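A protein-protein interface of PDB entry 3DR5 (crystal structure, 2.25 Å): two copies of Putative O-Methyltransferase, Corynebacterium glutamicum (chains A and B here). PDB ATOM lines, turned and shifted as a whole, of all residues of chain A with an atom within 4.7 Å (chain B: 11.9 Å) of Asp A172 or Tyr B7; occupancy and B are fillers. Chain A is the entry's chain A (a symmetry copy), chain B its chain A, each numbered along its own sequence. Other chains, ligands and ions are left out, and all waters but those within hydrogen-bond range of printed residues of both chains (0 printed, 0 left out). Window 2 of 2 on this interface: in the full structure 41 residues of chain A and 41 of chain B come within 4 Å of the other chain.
No position is printed for both chains.
Of the 4 pairs that touch across the chains among the printed residues, none has its exchanged pair printed and touching as well.
Of chain B, only Leu B8 comes within 4 Å of Gly A168.
No residue of chain B comes within 4 Å of Thr A169.
Printed residues of chain B within 4 Å of Ile A170: Tyr B11 (3.3 Å).
No residue of chain B comes within 4 Å of Gln A173.
No residue of chain B comes within 4 Å of Arg A175.
Of chain A, only Asp A172 (3.5 Å) comes within 4 Å of Tyr B7.
Printed residues of chain A within 4 Å of Leu B8: Gly A168.
Thr B10 touches none of the printed residues of chain A.
Of the printed residues of chain A, Tyr B11 touches Ile A170 and Ala A171.
Met B40 touches none of the printed residues of chain A.
The nearest residue of chain B that does not touch Asp A172 is Tyr B11 (6.5 Å).
The nearest printed residue of chain A that does not touch Leu B8 is Asp A167 (4.2 Å).
Of the 17 printed residues of chain B, 3 touch a printed residue of chain A.
Hydrophobic or aromatic side chains of chain B within 4 Å of the printed part of chain A: Tyr B7, Leu B8 and Tyr B11.
Hydrophobic or aromatic side chains of chain A that line the printed part of chain B: Ile A170 and Ala A171.
Among the printed residues, 4 pairs touch across the chains.
Among the printed residues, pairs that only touch across the chains: Gly A168 with Leu B8, Ile A170 with Tyr B11 and Ala A171 with Tyr B11.
OH of Tyr B7 is in hydrogen-bond range of OD2 of Asp A172 (3.5 Å).
The backbone carbonyl oxygen (O) of Tyr B11 sits at hydrogen-bond distance from the side-chain hydroxyl (OG) of Ser B14.
N of Ala A171 sits close to NH1 of Arg A184 (2.4 Å).
The side-chain hydroxyl (OG1) of Thr A174 sits at hydrogen-bond distance from the side-chain carboxylate (OD1) of Asp A172, 3.0 Å away.
The side-chain carboxylate of Asp A172 lies within salt-bridge range of the guanidinium group of Arg A175 (3.8 Å).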
ATOM      1  N   ASP A 167     -17.894 -19.189   6.122  1.00  0.00           N
ATOM      2  CA  ASP A 167     -18.590 -18.769   7.330  1.00  0.00           C
ATOM      3  C   ASP A 167     -18.743 -17.259   7.496  1.00  0.00           C
ATOM      4  O   ASP A 167     -18.988 -16.769   8.603  1.00  0.00           O
ATOM      5  CB  ASP A 167     -17.864 -19.347   8.546  1.00  0.00           C
ATOM      6  CG  ASP A 167     -18.066 -20.846   8.692  1.00  0.00           C
ATOM      7  OD1 ASP A 167     -19.235 -21.277   8.715  1.00  0.00           O
ATOM      8  OD2 ASP A 167     -17.067 -21.591   8.798  1.00  0.00           O
ATOM      9  N   GLY A 168     -18.602 -16.531   6.391  1.00  0.00           N
ATOM     10  CA  GLY A 168     -18.707 -15.087   6.433  1.00  0.00           C
ATOM     11  C   GLY A 168     -17.340 -14.464   6.667  1.00  0.00           C
ATOM     12  O   GLY A 168     -17.177 -13.246   6.596  1.00  0.00           O
ATOM     13  N   THR A 169     -16.355 -15.309   6.956  1.00  0.00           N
ATOM     14  CA  THR A 169     -14.978 -14.879   7.206  1.00  0.00           C
ATOM     15  C   THR A 169     -14.548 -13.722   6.317  1.00  0.00           C
ATOM     16  O   THR A 169     -13.824 -12.829   6.768  1.00  0.00           O
ATOM     17  CB  THR A 169     -13.986 -16.057   6.992  1.00  0.00           C
ATOM     18  OG1 THR A 169     -13.923 -16.863   8.176  1.00  0.00           O
ATOM     19  CG2 THR A 169     -12.592 -15.552   6.637  1.00  0.00           C
ATOM     20  N   ILE A 170     -14.989 -13.734   5.059  1.00  0.00           N
ATOM     21  CA  ILE A 170     -14.598 -12.684   4.125  1.00  0.00           C
ATOM     22  C   ILE A 170     -15.086 -11.291   4.533  1.00  0.00           C
ATOM     23  O   ILE A 170     -15.886 -11.154   5.453  1.00  0.00           O
ATOM     24  CB  ILE A 170     -15.000 -13.053   2.658  1.00  0.00           C
ATOM     25  CG1 ILE A 170     -16.475 -13.411   2.569  1.00  0.00           C
ATOM     26  CG2 ILE A 170     -14.148 -14.244   2.190  1.00  0.00           C
ATOM     27  CD1 ILE A 170     -16.877 -13.945   1.210  1.00  0.00           C
ATOM     28  N   ALA A 171     -14.596 -10.265   3.842  1.00  0.00           N
ATOM     29  CA  ALA A 171     -14.891  -8.865   4.164  1.00  0.00           C
ATOM     30  C   ALA A 171     -14.502  -8.648   5.633  1.00  0.00           C
ATOM     31  O   ALA A 171     -15.343  -8.309   6.475  1.00  0.00           O
ATOM     32  CB  ALA A 171     -16.360  -8.543   3.965  1.00  0.00           C
ATOM     33  N   ASP A 172     -13.220  -8.836   5.942  1.00  0.00           N
ATOM     34  CA  ASP A 172     -12.724  -8.666   7.308  1.00  0.00           C
ATOM     35  C   ASP A 172     -11.264  -8.223   7.252  1.00  0.00           C
ATOM     36  O   ASP A 172     -10.390  -8.983   6.836  1.00  0.00           O
ATOM     37  CB  ASP A 172     -12.834  -9.995   8.060  1.00  0.00           C
ATOM     38  CG  ASP A 172     -12.923  -9.827   9.559  1.00  0.00           C
ATOM     39  OD1 ASP A 172     -12.302  -8.893  10.095  1.00  0.00           O
ATOM     40  OD2 ASP A 172     -13.605 -10.647  10.206  1.00  0.00           O
ATOM     41  N   GLN A 173     -11.008  -6.995   7.688  1.00  0.00           N
ATOM     42  CA  GLN A 173      -9.662  -6.438   7.671  1.00  0.00           C
ATOM     43  C   GLN A 173      -8.614  -7.356   8.273  1.00  0.00           C
ATOM     44  O   GLN A 173      -7.591  -7.631   7.655  1.00  0.00           O
ATOM     45  CB  GLN A 173      -9.635  -5.082   8.390  1.00  0.00           C
ATOM     46  CG  GLN A 173     -10.352  -3.947   7.649  1.00  0.00           C
ATOM     47  CD  GLN A 173     -11.854  -4.146   7.559  1.00  0.00           C
ATOM     48  OE1 GLN A 173     -12.494  -4.527   8.535  1.00  0.00           O
ATOM     49  NE2 GLN A 173     -12.427  -3.870   6.390  1.00  0.00           N
ATOM     50  N   THR A 174      -8.881  -7.843   9.477  1.00  0.00           N
ATOM     51  CA  THR A 174      -7.952  -8.733  10.163  1.00  0.00           C
ATOM     52  C   THR A 174      -7.612  -9.954   9.331  1.00  0.00           C
ATOM     53  O   THR A 174      -6.440 -10.296   9.151  1.00  0.00           O
ATOM     54  CB  THR A 174      -8.519  -9.225  11.523  1.00  0.00           C
ATOM     55  OG1 THR A 174      -9.762  -9.914  11.312  1.00  0.00           O
ATOM     56  CG2 THR A 174      -8.738  -8.060  12.478  1.00  0.00           C
ATOM     57  N   ARG A 175      -8.650 -10.597   8.807  1.00  0.00           N
ATOM     58  CA  ARG A 175      -8.465 -11.814   8.027  1.00  0.00           C
ATOM     59  C   ARG A 175      -7.749 -11.712   6.687  1.00  0.00           C
ATOM     60  O   ARG A 175      -8.400 -11.677   5.641  1.00  0.00           O
ATOM     61  CB  ARG A 175      -9.814 -12.513   7.832  1.00  0.00           C
ATOM     62  CG  ARG A 175      -9.741 -14.044   7.709  1.00  0.00           C
ATOM     63  CD  ARG A 175      -9.879 -14.712   9.070  1.00  0.00           C
ATOM     64  NE  ARG A 175     -10.982 -14.133   9.837  1.00  0.00           N
ATOM     65  CZ  ARG A 175     -11.645 -14.771  10.798  1.00  0.00           C
ATOM     66  NH1 ARG A 175     -11.328 -16.020  11.116  1.00  0.00           N
ATOM     67  NH2 ARG A 175     -12.638 -14.159  11.435  1.00  0.00           N
ATOM     68  N   ARG A 184     -13.034 -14.225  -1.592  1.00  0.00           N
ATOM     69  CA  ARG A 184     -13.592 -12.877  -1.743  1.00  0.00           C
ATOM     70  C   ARG A 184     -13.673 -12.494  -3.225  1.00  0.00           C
ATOM     71  O   ARG A 184     -14.686 -11.951  -3.674  1.00  0.00           O
ATOM     72  CB  ARG A 184     -12.733 -11.847  -1.011  1.00  0.00           C
ATOM     73  CG  ARG A 184     -13.545 -10.776  -0.298  1.00  0.00           C
ATOM     74  CD  ARG A 184     -12.730  -9.526  -0.012  1.00  0.00           C
ATOM     75  NE  ARG A 184     -11.520  -9.793   0.760  1.00  0.00           N
ATOM     76  CZ  ARG A 184     -11.504 -10.374   1.956  1.00  0.00           C
ATOM     77  NH1 ARG A 184     -12.634 -10.752   2.526  1.00  0.00           N
ATOM     78  NH2 ARG A 184     -10.353 -10.576   2.586  1.00  0.00           N
ATOM     79  N   ASN B   3     -24.790 -16.897  16.414  1.00  0.00           N
ATOM     80  CA  ASN B   3     -23.530 -16.144  16.142  1.00  0.00           C
ATOM     81  C   ASN B   3     -23.121 -16.125  14.676  1.00  0.00           C
ATOM     82  O   ASN B   3     -23.217 -15.095  14.004  1.00  0.00           O
ATOM     83  CB  ASN B   3     -22.381 -16.718  16.990  1.00  0.00           C
ATOM     84  N   ALA B   4     -22.674 -17.274  14.182  1.00  0.00           N
ATOM     85  CA  ALA B   4     -22.187 -17.377  12.815  1.00  0.00           C
ATOM     86  C   ALA B   4     -23.199 -17.141  11.711  1.00  0.00           C
ATOM     87  O   ALA B   4     -22.845 -16.741  10.602  1.00  0.00           O
ATOM     88  CB  ALA B   4     -21.472 -18.723  12.615  1.00  0.00           C
ATOM     89  N   PHE B   5     -24.462 -17.368  12.032  1.00  0.00           N
ATOM     90  CA  PHE B   5     -25.536 -17.158  11.081  1.00  0.00           C
ATOM     91  C   PHE B   5     -25.606 -15.688  10.651  1.00  0.00           C
ATOM     92  O   PHE B   5     -25.813 -15.390   9.475  1.00  0.00           O
ATOM     93  CB  PHE B   5     -26.870 -17.545  11.711  1.00  0.00           C
ATOM     94  CG  PHE B   5     -28.067 -17.265  10.831  1.00  0.00           C
ATOM     95  CD1 PHE B   5     -28.466 -18.183   9.865  1.00  0.00           C
ATOM     96  CD2 PHE B   5     -28.777 -16.071  10.950  1.00  0.00           C
ATOM     97  CE1 PHE B   5     -29.552 -17.919   9.033  1.00  0.00           C
ATOM     98  CE2 PHE B   5     -29.861 -15.798  10.121  1.00  0.00           C
ATOM     99  CZ  PHE B   5     -30.249 -16.724   9.161  1.00  0.00           C
ATOM    100  N   GLU B   6     -25.437 -14.773  11.605  1.00  0.00           N
ATOM    101  CA  GLU B   6     -25.548 -13.343  11.334  1.00  0.00           C
ATOM    102  C   GLU B   6     -24.378 -12.707  10.606  1.00  0.00           C
ATOM    103  O   GLU B   6     -24.571 -11.751   9.852  1.00  0.00           O
ATOM    104  CB  GLU B   6     -25.825 -12.595  12.640  1.00  0.00           C
ATOM    105  CG  GLU B   6     -27.002 -13.152  13.442  1.00  0.00           C
ATOM    106  CD  GLU B   6     -26.647 -13.337  14.904  1.00  0.00           C
ATOM    107  OE1 GLU B   6     -25.879 -14.274  15.211  1.00  0.00           O
ATOM    108  OE2 GLU B   6     -27.122 -12.541  15.742  1.00  0.00           O
ATOM    109  N   TYR B   7     -23.179 -13.237  10.827  1.00  0.00           N
ATOM    110  CA  TYR B   7     -22.003 -12.730  10.148  1.00  0.00           C
ATOM    111  C   TYR B   7     -22.167 -13.141   8.677  1.00  0.00           C
ATOM    112  O   TYR B   7     -21.805 -12.395   7.764  1.00  0.00           O
ATOM    113  CB  TYR B   7     -20.727 -13.335  10.749  1.00  0.00           C
ATOM    114  CG  TYR B   7     -19.628 -12.313  10.922  1.00  0.00           C
ATOM    115  CD1 TYR B   7     -18.622 -12.501  11.863  1.00  0.00           C
ATOM    116  CD2 TYR B   7     -19.604 -11.143  10.151  1.00  0.00           C
ATOM    117  CE1 TYR B   7     -17.613 -11.554  12.040  1.00  0.00           C
ATOM    118  CE2 TYR B   7     -18.598 -10.191  10.318  1.00  0.00           C
ATOM    119  CZ  TYR B   7     -17.608 -10.404  11.265  1.00  0.00           C
ATOM    120  OH  TYR B   7     -16.614  -9.468  11.435  1.00  0.00           O
ATOM    121  N   LEU B   8     -22.712 -14.336   8.446  1.00  0.00           N
ATOM    122  CA  LEU B   8     -22.966 -14.797   7.084  1.00  0.00           C
ATOM    123  C   LEU B   8     -24.085 -13.876   6.550  1.00  0.00           C
ATOM    124  O   LEU B   8     -23.975 -13.318   5.457  1.00  0.00           O
ATOM    125  CB  LEU B   8     -23.447 -16.256   7.085  1.00  0.00           C
ATOM    126  CG  LEU B   8     -23.276 -17.036   5.778  1.00  0.00           C
ATOM    127  CD1 LEU B   8     -22.041 -16.535   5.032  1.00  0.00           C
ATOM    128  CD2 LEU B   8     -23.135 -18.521   6.097  1.00  0.00           C
ATOM    129  N   ARG B   9     -25.159 -13.709   7.324  1.00  0.00           N
ATOM    130  CA  ARG B   9     -26.273 -12.860   6.899  1.00  0.00           C
ATOM    131  C   ARG B   9     -25.805 -11.437   6.623  1.00  0.00           C
ATOM    132  O   ARG B   9     -26.133 -10.854   5.585  1.00  0.00           O
ATOM    133  CB  ARG B   9     -27.397 -12.870   7.952  1.00  0.00           C
ATOM    134  CG  ARG B   9     -28.589 -11.993   7.597  1.00  0.00           C
ATOM    135  CD  ARG B   9     -29.884 -12.551   8.167  1.00  0.00           C
ATOM    136  NE  ARG B   9     -29.857 -12.682   9.620  1.00  0.00           N
ATOM    137  CZ  ARG B   9     -29.949 -11.663  10.472  1.00  0.00           C
ATOM    138  NH1 ARG B   9     -30.079 -10.423  10.017  1.00  0.00           N
ATOM    139  NH2 ARG B   9     -29.912 -11.886  11.778  1.00  0.00           N
ATOM    140  N   THR B  10     -25.025 -10.888   7.548  1.00  0.00           N
ATOM    141  CA  THR B  10     -24.516  -9.531   7.411  1.00  0.00           C
ATOM    142  C   THR B  10     -23.670  -9.354   6.153  1.00  0.00           C
ATOM    143  O   THR B  10     -23.850  -8.392   5.406  1.00  0.00           O
ATOM    144  CB  THR B  10     -23.694  -9.122   8.655  1.00  0.00           C
ATOM    145  OG1 THR B  10     -24.506  -9.274   9.830  1.00  0.00           O
ATOM    146  CG2 THR B  10     -23.250  -7.676   8.545  1.00  0.00           C
ATOM    147  N   TYR B  11     -22.750 -10.281   5.915  1.00  0.00           N
ATOM    148  CA  TYR B  11     -21.909 -10.198   4.726  1.00  0.00           C
ATOM    149  C   TYR B  11     -22.738 -10.337   3.448  1.00  0.00           C
ATOM    150  O   TYR B  11     -22.509  -9.621   2.473  1.00  0.00           O
ATOM    151  CB  TYR B  11     -20.849 -11.287   4.713  1.00  0.00           C
ATOM    152  CG  TYR B  11     -20.011 -11.215   3.462  1.00  0.00           C
ATOM    153  CD1 TYR B  11     -19.074 -10.200   3.298  1.00  0.00           C
ATOM    154  CD2 TYR B  11     -20.233 -12.088   2.393  1.00  0.00           C
ATOM    155  CE1 TYR B  11     -18.368 -10.055   2.110  1.00  0.00           C
ATOM    156  CE2 TYR B  11     -19.529 -11.953   1.198  1.00  0.00           C
ATOM    157  CZ  TYR B  11     -18.602 -10.928   1.066  1.00  0.00           C
ATOM    158  OH  TYR B  11     -17.893 -10.787  -0.100  1.00  0.00           O
ATOM    159  N   VAL B  12     -23.698 -11.258   3.444  1.00  0.00           N
ATOM    160  CA  VAL B  12     -24.528 -11.461   2.261  1.00  0.00           C
ATOM    161  C   VAL B  12     -25.482 -10.294   2.040  1.00  0.00           C
ATOM    162  O   VAL B  12     -25.667  -9.845   0.910  1.00  0.00           O
ATOM    163  CB  VAL B  12     -25.335 -12.779   2.354  1.00  0.00           C
ATOM    164  CG1 VAL B  12     -26.306 -12.894   1.177  1.00  0.00           C
ATOM    165  CG2 VAL B  12     -24.375 -13.975   2.369  1.00  0.00           C
ATOM    166  N   GLU B  13     -26.094  -9.807   3.111  1.00  0.00           N
ATOM    167  CA  GLU B  13     -27.010  -8.686   2.983  1.00  0.00           C
ATOM    168  C   GLU B  13     -26.234  -7.423   2.605  1.00  0.00           C
ATOM    169  O   GLU B  13     -26.598  -6.715   1.672  1.00  0.00           O
ATOM    170  CB  GLU B  13     -27.791  -8.474   4.290  1.00  0.00           C
ATOM    171  CG  GLU B  13     -29.089  -9.277   4.362  1.00  0.00           C
ATOM    172  CD  GLU B  13     -29.825  -9.117   5.677  1.00  0.00           C
ATOM    173  OE1 GLU B  13     -30.776  -9.891   5.930  1.00  0.00           O
ATOM    174  OE2 GLU B  13     -29.460  -8.212   6.457  1.00  0.00           O
ATOM    175  N   SER B  14     -25.146  -7.154   3.319  1.00  0.00           N
ATOM    176  CA  SER B  14     -24.332  -5.965   3.068  1.00  0.00           C
ATOM    177  C   SER B  14     -23.584  -6.030   1.747  1.00  0.00           C
ATOM    178  O   SER B  14     -22.868  -5.088   1.393  1.00  0.00           O
ATOM    179  CB  SER B  14     -23.312  -5.785   4.188  1.00  0.00           C
ATOM    180  OG  SER B  14     -22.244  -6.722   4.062  1.00  0.00           O
ATOM    181  N   THR B  15     -23.756  -7.126   1.013  1.00  0.00           N
ATOM    182  CA  THR B  15     -23.033  -7.294  -0.234  1.00  0.00           C
ATOM    183  C   THR B  15     -23.896  -7.581  -1.460  1.00  0.00           C
ATOM    184  O   THR B  15     -23.396  -7.611  -2.588  1.00  0.00           O
ATOM    185  CB  THR B  15     -21.939  -8.384  -0.030  1.00  0.00           C
ATOM    186  OG1 THR B  15     -20.726  -7.984  -0.673  1.00  0.00           O
ATOM    187  CG2 THR B  15     -22.368  -9.696  -0.559  1.00  0.00           C
ATOM    188  N   THR B  16     -25.187  -7.806  -1.236  1.00  0.00           N
ATOM    189  CA  THR B  16     -26.114  -8.045  -2.336  1.00  0.00           C
ATOM    190  C   THR B  16     -26.468  -6.688  -2.968  1.00  0.00           C
ATOM    191  O   THR B  16     -26.960  -5.778  -2.287  1.00  0.00           O
ATOM    192  CB  THR B  16     -27.414  -8.718  -1.854  1.00  0.00           C
ATOM    193  OG1 THR B  16     -27.128 -10.043  -1.396  1.00  0.00           O
ATOM    194  CG2 THR B  16     -28.431  -8.788  -2.983  1.00  0.00           C
ATOM    195  N   ASP B  38     -36.449 -12.569   4.647  1.00  0.00           N
ATOM    196  CA  ASP B  38     -35.215 -11.804   4.478  1.00  0.00           C
ATOM    197  C   ASP B  38     -34.653 -11.927   3.059  1.00  0.00           C
ATOM    198  O   ASP B  38     -35.200 -12.647   2.222  1.00  0.00           O
ATOM    199  CB  ASP B  38     -34.164 -12.214   5.542  1.00  0.00           C
ATOM    200  CG  ASP B  38     -33.685 -13.652   5.401  1.00  0.00           C
ATOM    201  OD1 ASP B  38     -34.288 -14.423   4.621  1.00  0.00           O
ATOM    202  OD2 ASP B  38     -32.691 -14.004   6.081  1.00  0.00           O
ATOM    203  N   MET B  40     -31.974 -13.395   1.882  1.00  0.00           N
ATOM    204  CA  MET B  40     -31.482 -14.715   1.524  1.00  0.00           C
ATOM    205  C   MET B  40     -32.616 -15.656   1.123  1.00  0.00           C
ATOM    206  O   MET B  40     -32.471 -16.453   0.191  1.00  0.00           O
ATOM    207  CB  MET B  40     -30.657 -15.312   2.683  1.00  0.00           C
ATOM    208  CG  MET B  40     -29.219 -14.769   2.791  1.00  0.00           C
ATOM    209  SD  MET B  40     -28.164 -15.689   4.173  1.00  0.00           S
ATOM    210  CE  MET B  40     -26.726 -14.446   4.380  1.00  0.00           C
ATOM    211  N   PRO B 202     -32.461 -23.652   7.108  1.00  0.00           N
ATOM    212  CA  PRO B 202     -32.227 -22.616   8.121  1.00  0.00           C
ATOM    213  C   PRO B 202     -32.453 -21.176   7.646  1.00  0.00           C
ATOM    214  O   PRO B 202     -31.585 -20.329   7.809  1.00  0.00           O
ATOM    215  CB  PRO B 202     -30.777 -22.862   8.527  1.00  0.00           C
ATOM    216  CG  PRO B 202     -30.141 -23.249   7.227  1.00  0.00           C
ATOM    217  CD  PRO B 202     -31.183 -24.204   6.609  1.00  0.00           C
